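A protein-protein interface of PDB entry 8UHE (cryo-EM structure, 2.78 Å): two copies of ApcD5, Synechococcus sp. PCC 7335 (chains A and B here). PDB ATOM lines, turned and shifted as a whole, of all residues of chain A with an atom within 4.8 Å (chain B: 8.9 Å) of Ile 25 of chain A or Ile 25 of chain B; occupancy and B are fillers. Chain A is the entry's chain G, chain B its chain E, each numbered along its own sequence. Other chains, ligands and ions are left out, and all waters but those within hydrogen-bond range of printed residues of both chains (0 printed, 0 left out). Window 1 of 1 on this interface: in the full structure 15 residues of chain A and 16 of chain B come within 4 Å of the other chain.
CD of Lys 21 of chain A touches CD1 of Leu 3 of chain B, 3.6 Å away. Glu 6 of chain B touches Lys 21 of chain A (CG to NZ, 3.8 Å). CG of Lys 21 of chain A touches O of Gly 96 of chain B (3.8 Å). Lys 21 of chain A touches Ser 97 of chain B (NZ to OG, 3.9 Å). CD1 of Ile 25 of chain A touches CG2 of Ile 25 of chain B, at 3.6 Å.
The backbone carbonyl oxygen of Gly 96 of chain B lies within hydrogen-bond range of the guanidinium group of Arg 24 of chain A. NH1 of Arg 24 of chain A is in salt-bridge range of OE1 of Glu 145 of chain B. NH1 of Arg 24 of chain A lies close to NH1 of Arg 36 of chain B (3.0 Å). The side-chain carboxylate (OD2) of Asp 28 of chain A lies close to the side-chain carboxylate (OD2) of Asp 28 of chain B.
The backbone carbonyl oxygen (O) of Asp 28 of chain B is in hydrogen-bond range of the side-chain hydroxyl (OG1) of Thr 32 of chain B. The guanidinium group (NE) of Arg 36 of chain B lies within hydrogen-bond range of the side-chain hydroxyl (OG1) of Thr 32 of chain B (3.1 Å). OD1 of Asp 28 of chain A lies close to O of Arg 24 of chain A (2.6 Å).
Lys 21 of chain A touches Leu 3 of chain B, but with the chains exchanged Leu 3 of chain A does not touch Lys 21 of chain B (4.02 Å). Ile 25 of chain A touches its own counterpart, Ile 25 of chain B. Asp 28 of chain B touches its own counterpart, Asp 28 of chain A.
Ile 25 of chain A touches just one residue of chain B: Ile 25. Of chain A, only Ile 25 comes within 4 Å of Ile 25 of chain B. Of the printed residues of chain A, Arg 36 of chain B touches Arg 24. Printed residues of chain B within 4 Å of Arg 24 of chain A: Arg 36, Gly 96 and Glu 145. Of the printed residues of chain A, Glu 145 of chain B touches Arg 24 (2.4 Å). Printed residues of chain A within 4 Å of Ser 97 of chain B: Lys 21 (3.9 Å). Printed residues of chain B within 4 Å of Asp 28 of chain A: Asp 28 (3.0 Å). Phe 26 of chain A touches none of the printed residues of chain B. Phe 26 of chain B touches none of the printed residues of chain A. The nearest residue of chain B that does not touch Ile 25 of chain A is Leu 3 of chain B (4.8 Å). The nearest printed residue of chain A that does not touch Ile 25 of chain B is Asp 28 of chain A (4.8 Å). The nearest printed residue of chain A that does not touch Asp 28 of chain B is Phe 29 of chain A (6.3 Å).
Along chain B the printed residues that touch a printed residue of chain A span positions 3 to 145.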
ATOM      1  N   LEU A   3     -12.973 -27.429  11.555  1.00  0.00           N
ATOM      2  CA  LEU A   3     -12.744 -27.848  12.937  1.00  0.00           C
ATOM      3  C   LEU A   3     -13.974 -28.532  13.524  1.00  0.00           C
ATOM      4  O   LEU A   3     -13.858 -29.517  14.268  1.00  0.00           O
ATOM      5  CB  LEU A   3     -12.348 -26.630  13.774  1.00  0.00           C
ATOM      6  CG  LEU A   3     -12.840 -26.449  15.214  1.00  0.00           C
ATOM      7  CD1 LEU A   3     -12.118 -27.369  16.193  1.00  0.00           C
ATOM      8  CD2 LEU A   3     -12.694 -24.999  15.628  1.00  0.00           C
ATOM      9  N   LEU A   7     -14.707 -32.145  15.276  1.00  0.00           N
ATOM     10  CA  LEU A   7     -15.416 -32.282  16.545  1.00  0.00           C
ATOM     11  C   LEU A   7     -16.514 -33.340  16.445  1.00  0.00           C
ATOM     12  O   LEU A   7     -16.632 -34.221  17.310  1.00  0.00           O
ATOM     13  CB  LEU A   7     -15.994 -30.925  16.939  1.00  0.00           C
ATOM     14  CG  LEU A   7     -15.714 -30.419  18.346  1.00  0.00           C
ATOM     15  CD1 LEU A   7     -14.252 -30.621  18.716  1.00  0.00           C
ATOM     16  CD2 LEU A   7     -16.052 -28.956  18.376  1.00  0.00           C
ATOM     17  N   LYS A  21     -16.920 -30.102  26.668  1.00  0.00           N
ATOM     18  CA  LYS A  21     -15.624 -29.551  26.294  1.00  0.00           C
ATOM     19  C   LYS A  21     -15.570 -29.255  24.799  1.00  0.00           C
ATOM     20  O   LYS A  21     -15.178 -28.156  24.390  1.00  0.00           O
ATOM     21  CB  LYS A  21     -14.517 -30.520  26.707  1.00  0.00           C
ATOM     22  CG  LYS A  21     -13.119 -30.103  26.296  1.00  0.00           C
ATOM     23  CD  LYS A  21     -12.173 -31.295  26.131  1.00  0.00           C
ATOM     24  CE  LYS A  21     -12.877 -32.586  25.739  1.00  0.00           C
ATOM     25  NZ  LYS A  21     -11.903 -33.708  25.665  1.00  0.00           N
ATOM     26  N   GLU A  22     -16.005 -30.215  23.974  1.00  0.00           N
ATOM     27  CA  GLU A  22     -16.109 -29.989  22.534  1.00  0.00           C
ATOM     28  C   GLU A  22     -17.131 -28.905  22.220  1.00  0.00           C
ATOM     29  O   GLU A  22     -16.948 -28.112  21.286  1.00  0.00           O
ATOM     30  CB  GLU A  22     -16.487 -31.290  21.830  1.00  0.00           C
ATOM     31  CG  GLU A  22     -15.618 -32.470  22.208  1.00  0.00           C
ATOM     32  CD  GLU A  22     -15.821 -33.662  21.297  1.00  0.00           C
ATOM     33  OE1 GLU A  22     -16.748 -33.630  20.460  1.00  0.00           O
ATOM     34  OE2 GLU A  22     -15.048 -34.634  21.418  1.00  0.00           O
ATOM     35  N   LEU A  23     -18.212 -28.851  22.997  1.00  0.00           N
ATOM     36  CA  LEU A  23     -19.177 -27.773  22.833  1.00  0.00           C
ATOM     37  C   LEU A  23     -18.540 -26.425  23.131  1.00  0.00           C
ATOM     38  O   LEU A  23     -18.825 -25.447  22.444  1.00  0.00           O
ATOM     39  CB  LEU A  23     -20.392 -28.019  23.723  1.00  0.00           C
ATOM     40  CG  LEU A  23     -21.151 -29.315  23.430  1.00  0.00           C
ATOM     41  CD1 LEU A  23     -22.437 -29.361  24.217  1.00  0.00           C
ATOM     42  CD2 LEU A  23     -21.441 -29.442  21.952  1.00  0.00           C
ATOM     43  N   ARG A  24     -17.643 -26.372  24.119  1.00  0.00           N
ATOM     44  CA  ARG A  24     -16.907 -25.150  24.423  1.00  0.00           C
ATOM     45  C   ARG A  24     -15.995 -24.759  23.272  1.00  0.00           C
ATOM     46  O   ARG A  24     -15.894 -23.583  22.941  1.00  0.00           O
ATOM     47  CB  ARG A  24     -16.101 -25.346  25.702  1.00  0.00           C
ATOM     48  CG  ARG A  24     -15.691 -24.088  26.432  1.00  0.00           C
ATOM     49  CD  ARG A  24     -15.351 -24.444  27.871  1.00  0.00           C
ATOM     50  NE  ARG A  24     -15.022 -25.860  27.997  1.00  0.00           N
ATOM     51  CZ  ARG A  24     -14.887 -26.505  29.147  1.00  0.00           C
ATOM     52  NH1 ARG A  24     -15.073 -25.896  30.306  1.00  0.00           N
ATOM     53  NH2 ARG A  24     -14.565 -27.795  29.134  1.00  0.00           N
ATOM     54  N   ILE A  25     -15.332 -25.731  22.642  1.00  0.00           N
ATOM     55  CA  ILE A  25     -14.546 -25.439  21.436  1.00  0.00           C
ATOM     56  C   ILE A  25     -15.433 -24.829  20.359  1.00  0.00           C
ATOM     57  O   ILE A  25     -15.050 -23.869  19.674  1.00  0.00           O
ATOM     58  CB  ILE A  25     -13.850 -26.708  20.903  1.00  0.00           C
ATOM     59  CG1 ILE A  25     -13.279 -27.563  22.028  1.00  0.00           C
ATOM     60  CG2 ILE A  25     -12.770 -26.356  19.895  1.00  0.00           C
ATOM     61  CD1 ILE A  25     -12.166 -26.934  22.774  1.00  0.00           C
ATOM     62  N   PHE A  26     -16.641 -25.378  20.212  1.00  0.00           N
ATOM     63  CA  PHE A  26     -17.602 -24.867  19.241  1.00  0.00           C
ATOM     64  C   PHE A  26     -18.020 -23.430  19.552  1.00  0.00           C
ATOM     65  O   PHE A  26     -18.102 -22.594  18.643  1.00  0.00           O
ATOM     66  CB  PHE A  26     -18.816 -25.793  19.201  1.00  0.00           C
ATOM     67  CG  PHE A  26     -19.773 -25.484  18.102  1.00  0.00           C
ATOM     68  CD1 PHE A  26     -19.316 -25.254  16.818  1.00  0.00           C
ATOM     69  CD2 PHE A  26     -21.132 -25.427  18.351  1.00  0.00           C
ATOM     70  CE1 PHE A  26     -20.197 -24.968  15.806  1.00  0.00           C
ATOM     71  CE2 PHE A  26     -22.015 -25.147  17.341  1.00  0.00           C
ATOM     72  CZ  PHE A  26     -21.549 -24.914  16.067  1.00  0.00           C
ATOM     73  N   GLN A  27     -18.278 -23.127  20.833  1.00  0.00           N
ATOM     74  CA  GLN A  27     -18.637 -21.760  21.229  1.00  0.00           C
ATOM     75  C   GLN A  27     -17.515 -20.783  20.904  1.00  0.00           C
ATOM     76  O   GLN A  27     -17.758 -19.691  20.368  1.00  0.00           O
ATOM     77  CB  GLN A  27     -18.947 -21.666  22.729  1.00  0.00           C
ATOM     78  CG  GLN A  27     -19.768 -22.757  23.375  1.00  0.00           C
ATOM     79  CD  GLN A  27     -21.250 -22.503  23.369  1.00  0.00           C
ATOM     80  OE1 GLN A  27     -22.030 -23.336  23.813  1.00  0.00           O
ATOM     81  NE2 GLN A  27     -21.648 -21.334  22.897  1.00  0.00           N
ATOM     82  N   ASP A  28     -16.276 -21.157  21.242  1.00  0.00           N
ATOM     83  CA  ASP A  28     -15.136 -20.267  21.034  1.00  0.00           C
ATOM     84  C   ASP A  28     -14.894 -19.998  19.558  1.00  0.00           C
ATOM     85  O   ASP A  28     -14.633 -18.856  19.156  1.00  0.00           O
ATOM     86  CB  ASP A  28     -13.896 -20.868  21.689  1.00  0.00           C
ATOM     87  CG  ASP A  28     -14.099 -21.130  23.159  1.00  0.00           C
ATOM     88  OD1 ASP A  28     -15.263 -21.192  23.587  1.00  0.00           O
ATOM     89  OD2 ASP A  28     -13.105 -21.290  23.891  1.00  0.00           O
ATOM     90  N   PHE A  29     -14.987 -21.040  18.734  1.00  0.00           N
ATOM     91  CA  PHE A  29     -14.871 -20.854  17.293  1.00  0.00           C
ATOM     92  C   PHE A  29     -16.006 -19.985  16.757  1.00  0.00           C
ATOM     93  O   PHE A  29     -15.799 -19.139  15.872  1.00  0.00           O
ATOM     94  CB  PHE A  29     -14.846 -22.223  16.623  1.00  0.00           C
ATOM     95  CG  PHE A  29     -14.836 -22.171  15.135  1.00  0.00           C
ATOM     96  CD1 PHE A  29     -15.858 -22.757  14.413  1.00  0.00           C
ATOM     97  CD2 PHE A  29     -13.814 -21.542  14.454  1.00  0.00           C
ATOM     98  CE1 PHE A  29     -15.861 -22.717  13.043  1.00  0.00           C
ATOM     99  CE2 PHE A  29     -13.822 -21.494  13.081  1.00  0.00           C
ATOM    100  CZ  PHE A  29     -14.839 -22.088  12.372  1.00  0.00           C
ATOM    101  N   SER B   2      -7.696 -34.283  30.910  1.00  0.00           N
ATOM    102  CA  SER B   2      -7.650 -32.827  30.877  1.00  0.00           C
ATOM    103  C   SER B   2      -7.555 -32.302  29.449  1.00  0.00           C
ATOM    104  O   SER B   2      -7.377 -33.072  28.505  1.00  0.00           O
ATOM    105  CB  SER B   2      -6.475 -32.313  31.708  1.00  0.00           C
ATOM    106  OG  SER B   2      -5.246 -32.826  31.229  1.00  0.00           O
ATOM    107  N   LEU B   3      -7.685 -30.982  29.300  1.00  0.00           N
ATOM    108  CA  LEU B   3      -7.650 -30.372  27.974  1.00  0.00           C
ATOM    109  C   LEU B   3      -6.253 -30.433  27.372  1.00  0.00           C
ATOM    110  O   LEU B   3      -6.100 -30.623  26.158  1.00  0.00           O
ATOM    111  CB  LEU B   3      -8.142 -28.926  28.057  1.00  0.00           C
ATOM    112  CG  LEU B   3      -8.594 -28.220  26.774  1.00  0.00           C
ATOM    113  CD1 LEU B   3      -9.222 -29.188  25.795  1.00  0.00           C
ATOM    114  CD2 LEU B   3      -9.568 -27.099  27.100  1.00  0.00           C
ATOM    115  N   VAL B   4      -5.224 -30.279  28.209  1.00  0.00           N
ATOM    116  CA  VAL B   4      -3.846 -30.267  27.729  1.00  0.00           C
ATOM    117  C   VAL B   4      -3.440 -31.644  27.217  1.00  0.00           C
ATOM    118  O   VAL B   4      -2.902 -31.772  26.112  1.00  0.00           O
ATOM    119  CB  VAL B   4      -2.902 -29.781  28.843  1.00  0.00           C
ATOM    120  CG1 VAL B   4      -1.463 -29.840  28.381  1.00  0.00           C
ATOM    121  CG2 VAL B   4      -3.272 -28.372  29.272  1.00  0.00           C
ATOM    122  N   GLU B   6      -5.386 -34.094  26.251  1.00  0.00           N
ATOM    123  CA  GLU B   6      -6.170 -34.422  25.062  1.00  0.00           C
ATOM    124  C   GLU B   6      -5.657 -33.680  23.838  1.00  0.00           C
ATOM    125  O   GLU B   6      -5.593 -34.252  22.743  1.00  0.00           O
ATOM    126  CB  GLU B   6      -7.650 -34.117  25.317  1.00  0.00           C
ATOM    127  CG  GLU B   6      -8.418 -35.221  26.064  1.00  0.00           C
ATOM    128  CD  GLU B   6      -7.971 -36.641  25.783  1.00  0.00           C
ATOM    129  OE1 GLU B   6      -7.760 -36.964  24.601  1.00  0.00           O
ATOM    130  OE2 GLU B   6      -7.814 -37.423  26.744  1.00  0.00           O
ATOM    131  N   LEU B   7      -5.262 -32.416  24.008  1.00  0.00           N
ATOM    132  CA  LEU B   7      -4.699 -31.656  22.896  1.00  0.00           C
ATOM    133  C   LEU B   7      -3.374 -32.248  22.429  1.00  0.00           C
ATOM    134  O   LEU B   7      -3.098 -32.300  21.224  1.00  0.00           O
ATOM    135  CB  LEU B   7      -4.517 -30.194  23.306  1.00  0.00           C
ATOM    136  CG  LEU B   7      -5.598 -29.176  22.931  1.00  0.00           C
ATOM    137  CD1 LEU B   7      -6.962 -29.826  22.723  1.00  0.00           C
ATOM    138  CD2 LEU B   7      -5.677 -28.100  24.000  1.00  0.00           C
ATOM    139  N   ALA B  19      -1.401 -27.732  16.409  1.00  0.00           N
ATOM    140  CA  ALA B  19      -1.928 -26.933  15.310  1.00  0.00           C
ATOM    141  C   ALA B  19      -2.467 -25.560  15.683  1.00  0.00           C
ATOM    142  O   ALA B  19      -2.665 -25.256  16.854  1.00  0.00           O
ATOM    143  CB  ALA B  19      -3.024 -27.715  14.584  1.00  0.00           C
ATOM    144  N   PRO B  20      -2.700 -24.717  14.678  1.00  0.00           N
ATOM    145  CA  PRO B  20      -3.228 -23.365  14.914  1.00  0.00           C
ATOM    146  C   PRO B  20      -4.459 -23.310  15.831  1.00  0.00           C
ATOM    147  O   PRO B  20      -4.714 -22.268  16.429  1.00  0.00           O
ATOM    148  CB  PRO B  20      -3.604 -22.908  13.506  1.00  0.00           C
ATOM    149  CG  PRO B  20      -2.640 -23.606  12.623  1.00  0.00           C
ATOM    150  CD  PRO B  20      -2.399 -24.949  13.255  1.00  0.00           C
ATOM    151  N   LYS B  21      -5.225 -24.392  15.956  1.00  0.00           N
ATOM    152  CA  LYS B  21      -6.340 -24.363  16.899  1.00  0.00           C
ATOM    153  C   LYS B  21      -5.969 -24.781  18.301  1.00  0.00           C
ATOM    154  O   LYS B  21      -6.535 -24.272  19.258  1.00  0.00           O
ATOM    155  CB  LYS B  21      -7.482 -25.273  16.443  1.00  0.00           C
ATOM    156  CG  LYS B  21      -7.790 -25.234  14.961  1.00  0.00           C
ATOM    157  CD  LYS B  21      -8.395 -26.556  14.524  1.00  0.00           C
ATOM    158  CE  LYS B  21      -7.555 -27.723  15.023  1.00  0.00           C
ATOM    159  NZ  LYS B  21      -6.146 -27.616  14.564  1.00  0.00           N
ATOM    160  N   GLU B  22      -5.051 -25.731  18.431  1.00  0.00           N
ATOM    161  CA  GLU B  22      -4.716 -26.309  19.732  1.00  0.00           C
ATOM    162  C   GLU B  22      -4.100 -25.280  20.670  1.00  0.00           C
ATOM    163  O   GLU B  22      -4.445 -25.221  21.857  1.00  0.00           O
ATOM    164  CB  GLU B  22      -3.788 -27.508  19.549  1.00  0.00           C
ATOM    165  CG  GLU B  22      -4.554 -28.806  19.386  1.00  0.00           C
ATOM    166  CD  GLU B  22      -3.880 -29.768  18.448  1.00  0.00           C
ATOM    167  OE1 GLU B  22      -2.930 -29.347  17.764  1.00  0.00           O
ATOM    168  OE2 GLU B  22      -4.303 -30.942  18.388  1.00  0.00           O
ATOM    169  N   LEU B  23      -3.183 -24.459  20.159  1.00  0.00           N
ATOM    170  CA  LEU B  23      -2.634 -23.385  20.976  1.00  0.00           C
ATOM    171  C   LEU B  23      -3.720 -22.386  21.352  1.00  0.00           C
ATOM    172  O   LEU B  23      -3.700 -21.840  22.454  1.00  0.00           O
ATOM    173  CB  LEU B  23      -1.490 -22.662  20.264  1.00  0.00           C
ATOM    174  CG  LEU B  23      -0.101 -23.305  20.210  1.00  0.00           C
ATOM    175  CD1 LEU B  23       0.145 -24.277  21.365  1.00  0.00           C
ATOM    176  CD2 LEU B  23       0.128 -23.979  18.878  1.00  0.00           C
ATOM    177  N   ARG B  24      -4.672 -22.151  20.447  1.00  0.00           N
ATOM    178  CA  ARG B  24      -5.767 -21.228  20.734  1.00  0.00           C
ATOM    179  C   ARG B  24      -6.652 -21.746  21.864  1.00  0.00           C
ATOM    180  O   ARG B  24      -7.031 -20.988  22.767  1.00  0.00           O
ATOM    181  CB  ARG B  24      -6.577 -20.997  19.460  1.00  0.00           C
ATOM    182  CG  ARG B  24      -7.904 -20.296  19.650  1.00  0.00           C
ATOM    183  CD  ARG B  24      -8.240 -19.495  18.409  1.00  0.00           C
ATOM    184  NE  ARG B  24      -7.340 -18.359  18.257  1.00  0.00           N
ATOM    185  CZ  ARG B  24      -7.732 -17.128  17.960  1.00  0.00           C
ATOM    186  NH1 ARG B  24      -9.001 -16.845  17.720  1.00  0.00           N
ATOM    187  NH2 ARG B  24      -6.827 -16.155  17.901  1.00  0.00           N
ATOM    188  N   ILE B  25      -6.968 -23.042  21.836  1.00  0.00           N
ATOM    189  CA  ILE B  25      -7.729 -23.660  22.921  1.00  0.00           C
ATOM    190  C   ILE B  25      -6.929 -23.631  24.218  1.00  0.00           C
ATOM    191  O   ILE B  25      -7.487 -23.422  25.304  1.00  0.00           O
ATOM    192  CB  ILE B  25      -8.144 -25.092  22.534  1.00  0.00           C
ATOM    193  CG1 ILE B  25      -8.996 -25.073  21.265  1.00  0.00           C
ATOM    194  CG2 ILE B  25      -8.878 -25.772  23.668  1.00  0.00           C
ATOM    195  CD1 ILE B  25     -10.199 -24.164  21.360  1.00  0.00           C
ATOM    196  N   PHE B  26      -5.609 -23.818  24.125  1.00  0.00           N
ATOM    197  CA  PHE B  26      -4.764 -23.736  25.313  1.00  0.00           C
ATOM    198  C   PHE B  26      -4.790 -22.336  25.922  1.00  0.00           C
ATOM    199  O   PHE B  26      -4.876 -22.186  27.147  1.00  0.00           O
ATOM    200  CB  PHE B  26      -3.334 -24.151  24.968  1.00  0.00           C
ATOM    201  CG  PHE B  26      -2.427 -24.221  26.160  1.00  0.00           C
ATOM    202  CD1 PHE B  26      -2.630 -25.172  27.144  1.00  0.00           C
ATOM    203  CD2 PHE B  26      -1.379 -23.326  26.305  1.00  0.00           C
ATOM    204  CE1 PHE B  26      -1.802 -25.232  28.249  1.00  0.00           C
ATOM    205  CE2 PHE B  26      -0.548 -23.384  27.410  1.00  0.00           C
ATOM    206  CZ  PHE B  26      -0.760 -24.336  28.382  1.00  0.00           C
ATOM    207  N   GLN B  27      -4.730 -21.300  25.080  1.00  0.00           N
ATOM    208  CA  GLN B  27      -4.816 -19.928  25.576  1.00  0.00           C
ATOM    209  C   GLN B  27      -6.178 -19.643  26.194  1.00  0.00           C
ATOM    210  O   GLN B  27      -6.264 -18.964  27.225  1.00  0.00           O
ATOM    211  CB  GLN B  27      -4.523 -18.925  24.459  1.00  0.00           C
ATOM    212  CG  GLN B  27      -3.156 -19.064  23.821  1.00  0.00           C
ATOM    213  CD  GLN B  27      -2.660 -17.768  23.225  1.00  0.00           C
ATOM    214  OE1 GLN B  27      -2.818 -16.700  23.815  1.00  0.00           O
ATOM    215  NE2 GLN B  27      -2.077 -17.849  22.034  1.00  0.00           N
ATOM    216  N   ASP B  28      -7.252 -20.157  25.581  1.00  0.00           N
ATOM    217  CA  ASP B  28      -8.583 -20.006  26.170  1.00  0.00           C
ATOM    218  C   ASP B  28      -8.653 -20.660  27.543  1.00  0.00           C
ATOM    219  O   ASP B  28      -9.211 -20.085  28.484  1.00  0.00           O
ATOM    220  CB  ASP B  28      -9.650 -20.603  25.251  1.00  0.00           C
ATOM    221  CG  ASP B  28      -9.741 -19.889  23.919  1.00  0.00           C
ATOM    222  OD1 ASP B  28      -9.173 -18.785  23.796  1.00  0.00           O
ATOM    223  OD2 ASP B  28     -10.386 -20.430  22.996  1.00  0.00           O
ATOM    224  N   PHE B  29      -8.065 -21.849  27.676  1.00  0.00           N
ATOM    225  CA  PHE B  29      -8.068 -22.568  28.945  1.00  0.00           C
ATOM    226  C   PHE B  29      -7.285 -21.811  30.001  1.00  0.00           C
ATOM    227  O   PHE B  29      -7.767 -21.633  31.132  1.00  0.00           O
ATOM    228  CB  PHE B  29      -7.504 -23.970  28.728  1.00  0.00           C
ATOM    229  CG  PHE B  29      -7.264 -24.747  29.987  1.00  0.00           C
ATOM    230  CD1 PHE B  29      -8.317 -25.124  30.802  1.00  0.00           C
ATOM    231  CD2 PHE B  29      -5.983 -25.144  30.328  1.00  0.00           C
ATOM    232  CE1 PHE B  29      -8.088 -25.855  31.951  1.00  0.00           C
ATOM    233  CE2 PHE B  29      -5.750 -25.877  31.472  1.00  0.00           C
ATOM    234  CZ  PHE B  29      -6.806 -26.242  32.280  1.00  0.00           C
ATOM    235  N   VAL B  30      -6.114 -21.273  29.618  1.00  0.00           N
ATOM    236  CA  VAL B  30      -5.286 -20.582  30.599  1.00  0.00           C
ATOM    237  C   VAL B  30      -5.879 -19.247  31.013  1.00  0.00           C
ATOM    238  O   VAL B  30      -5.708 -18.797  32.158  1.00  0.00           O
ATOM    239  CB  VAL B  30      -3.803 -20.478  30.196  1.00  0.00           C
ATOM    240  CG1 VAL B  30      -3.229 -21.879  29.933  1.00  0.00           C
ATOM    241  CG2 VAL B  30      -3.619 -19.530  29.089  1.00  0.00           C
ATOM    242  N   LYS B  31      -6.616 -18.610  30.116  1.00  0.00           N
ATOM    243  CA  LYS B  31      -7.196 -17.328  30.456  1.00  0.00           C
ATOM    244  C   LYS B  31      -8.533 -17.476  31.168  1.00  0.00           C
ATOM    245  O   LYS B  31      -8.930 -16.574  31.914  1.00  0.00           O
ATOM    246  CB  LYS B  31      -7.325 -16.474  29.197  1.00  0.00           C
ATOM    247  CG  LYS B  31      -5.977 -15.986  28.674  1.00  0.00           C
ATOM    248  CD  LYS B  31      -6.023 -15.669  27.191  1.00  0.00           C
ATOM    249  CE  LYS B  31      -4.680 -15.161  26.696  1.00  0.00           C
ATOM    250  NZ  LYS B  31      -4.445 -15.544  25.276  1.00  0.00           N
ATOM    251  N   THR B  32      -9.233 -18.593  30.970  1.00  0.00           N
ATOM    252  CA  THR B  32     -10.397 -18.914  31.787  1.00  0.00           C
ATOM    253  C   THR B  32     -10.018 -19.634  33.071  1.00  0.00           C
ATOM    254  O   THR B  32     -10.910 -20.015  33.842  1.00  0.00           O
ATOM    255  CB  THR B  32     -11.389 -19.767  30.992  1.00  0.00           C
ATOM    256  OG1 THR B  32     -10.727 -20.936  30.493  1.00  0.00           O
ATOM    257  CG2 THR B  32     -11.959 -18.970  29.831  1.00  0.00           C
ATOM    258  N   GLY B  33      -8.720 -19.852  33.286  1.00  0.00           N
ATOM    259  CA  GLY B  33      -8.268 -20.492  34.508  1.00  0.00           C
ATOM    260  C   GLY B  33      -8.643 -19.775  35.785  1.00  0.00           C
ATOM    261  O   GLY B  33      -8.915 -20.419  36.797  1.00  0.00           O
ATOM    262  N   ARG B  36     -12.140 -20.705  36.460  1.00  0.00           N
ATOM    263  CA  ARG B  36     -12.201 -22.105  36.880  1.00  0.00           C
ATOM    264  C   ARG B  36     -11.749 -22.284  38.327  1.00  0.00           C
ATOM    265  O   ARG B  36     -12.350 -23.057  39.086  1.00  0.00           O
ATOM    266  CB  ARG B  36     -11.356 -22.969  35.946  1.00  0.00           C
ATOM    267  CG  ARG B  36     -11.877 -22.997  34.529  1.00  0.00           C
ATOM    268  CD  ARG B  36     -10.893 -23.634  33.567  1.00  0.00           C
ATOM    269  NE  ARG B  36     -11.340 -23.497  32.186  1.00  0.00           N
ATOM    270  CZ  ARG B  36     -12.300 -24.225  31.631  1.00  0.00           C
ATOM    271  NH1 ARG B  36     -12.939 -25.164  32.311  1.00  0.00           N
ATOM    272  NH2 ARG B  36     -12.624 -24.009  30.360  1.00  0.00           N
ATOM    273  N   GLY B  96     -10.245 -28.533  32.926  1.00  0.00           N
ATOM    274  CA  GLY B  96     -10.768 -28.105  31.651  1.00  0.00           C
ATOM    275  C   GLY B  96     -11.457 -29.188  30.859  1.00  0.00           C
ATOM    276  O   GLY B  96     -11.957 -28.909  29.763  1.00  0.00           O
ATOM    277  N   SER B  97     -11.514 -30.409  31.382  1.00  0.00           N
ATOM    278  CA  SER B  97     -12.125 -31.524  30.681  1.00  0.00           C
ATOM    279  C   SER B  97     -12.686 -32.497  31.703  1.00  0.00           C
ATOM    280  O   SER B  97     -12.192 -32.591  32.830  1.00  0.00           O
ATOM    281  CB  SER B  97     -11.118 -32.226  29.767  1.00  0.00           C
ATOM    282  OG  SER B  97     -11.488 -33.573  29.536  1.00  0.00           O
ATOM    283  N   GLU B 145     -20.942 -24.070  33.406  1.00  0.00           N
ATOM    284  CA  GLU B 145     -19.777 -24.949  33.327  1.00  0.00           C
ATOM    285  C   GLU B 145     -19.899 -26.126  34.287  1.00  0.00           C
ATOM    286  O   GLU B 145     -19.409 -27.223  33.997  1.00  0.00           O
ATOM    287  CB  GLU B 145     -18.493 -24.167  33.607  1.00  0.00           C
ATOM    288  CG  GLU B 145     -18.037 -23.260  32.473  1.00  0.00           C
ATOM    289  CD  GLU B 145     -17.732 -24.023  31.191  1.00  0.00           C
ATOM    290  OE1 GLU B 145     -17.176 -25.139  31.271  1.00  0.00           O
ATOM    291  OE2 GLU B 145     -18.041 -23.498  30.101  1.00  0.00           O
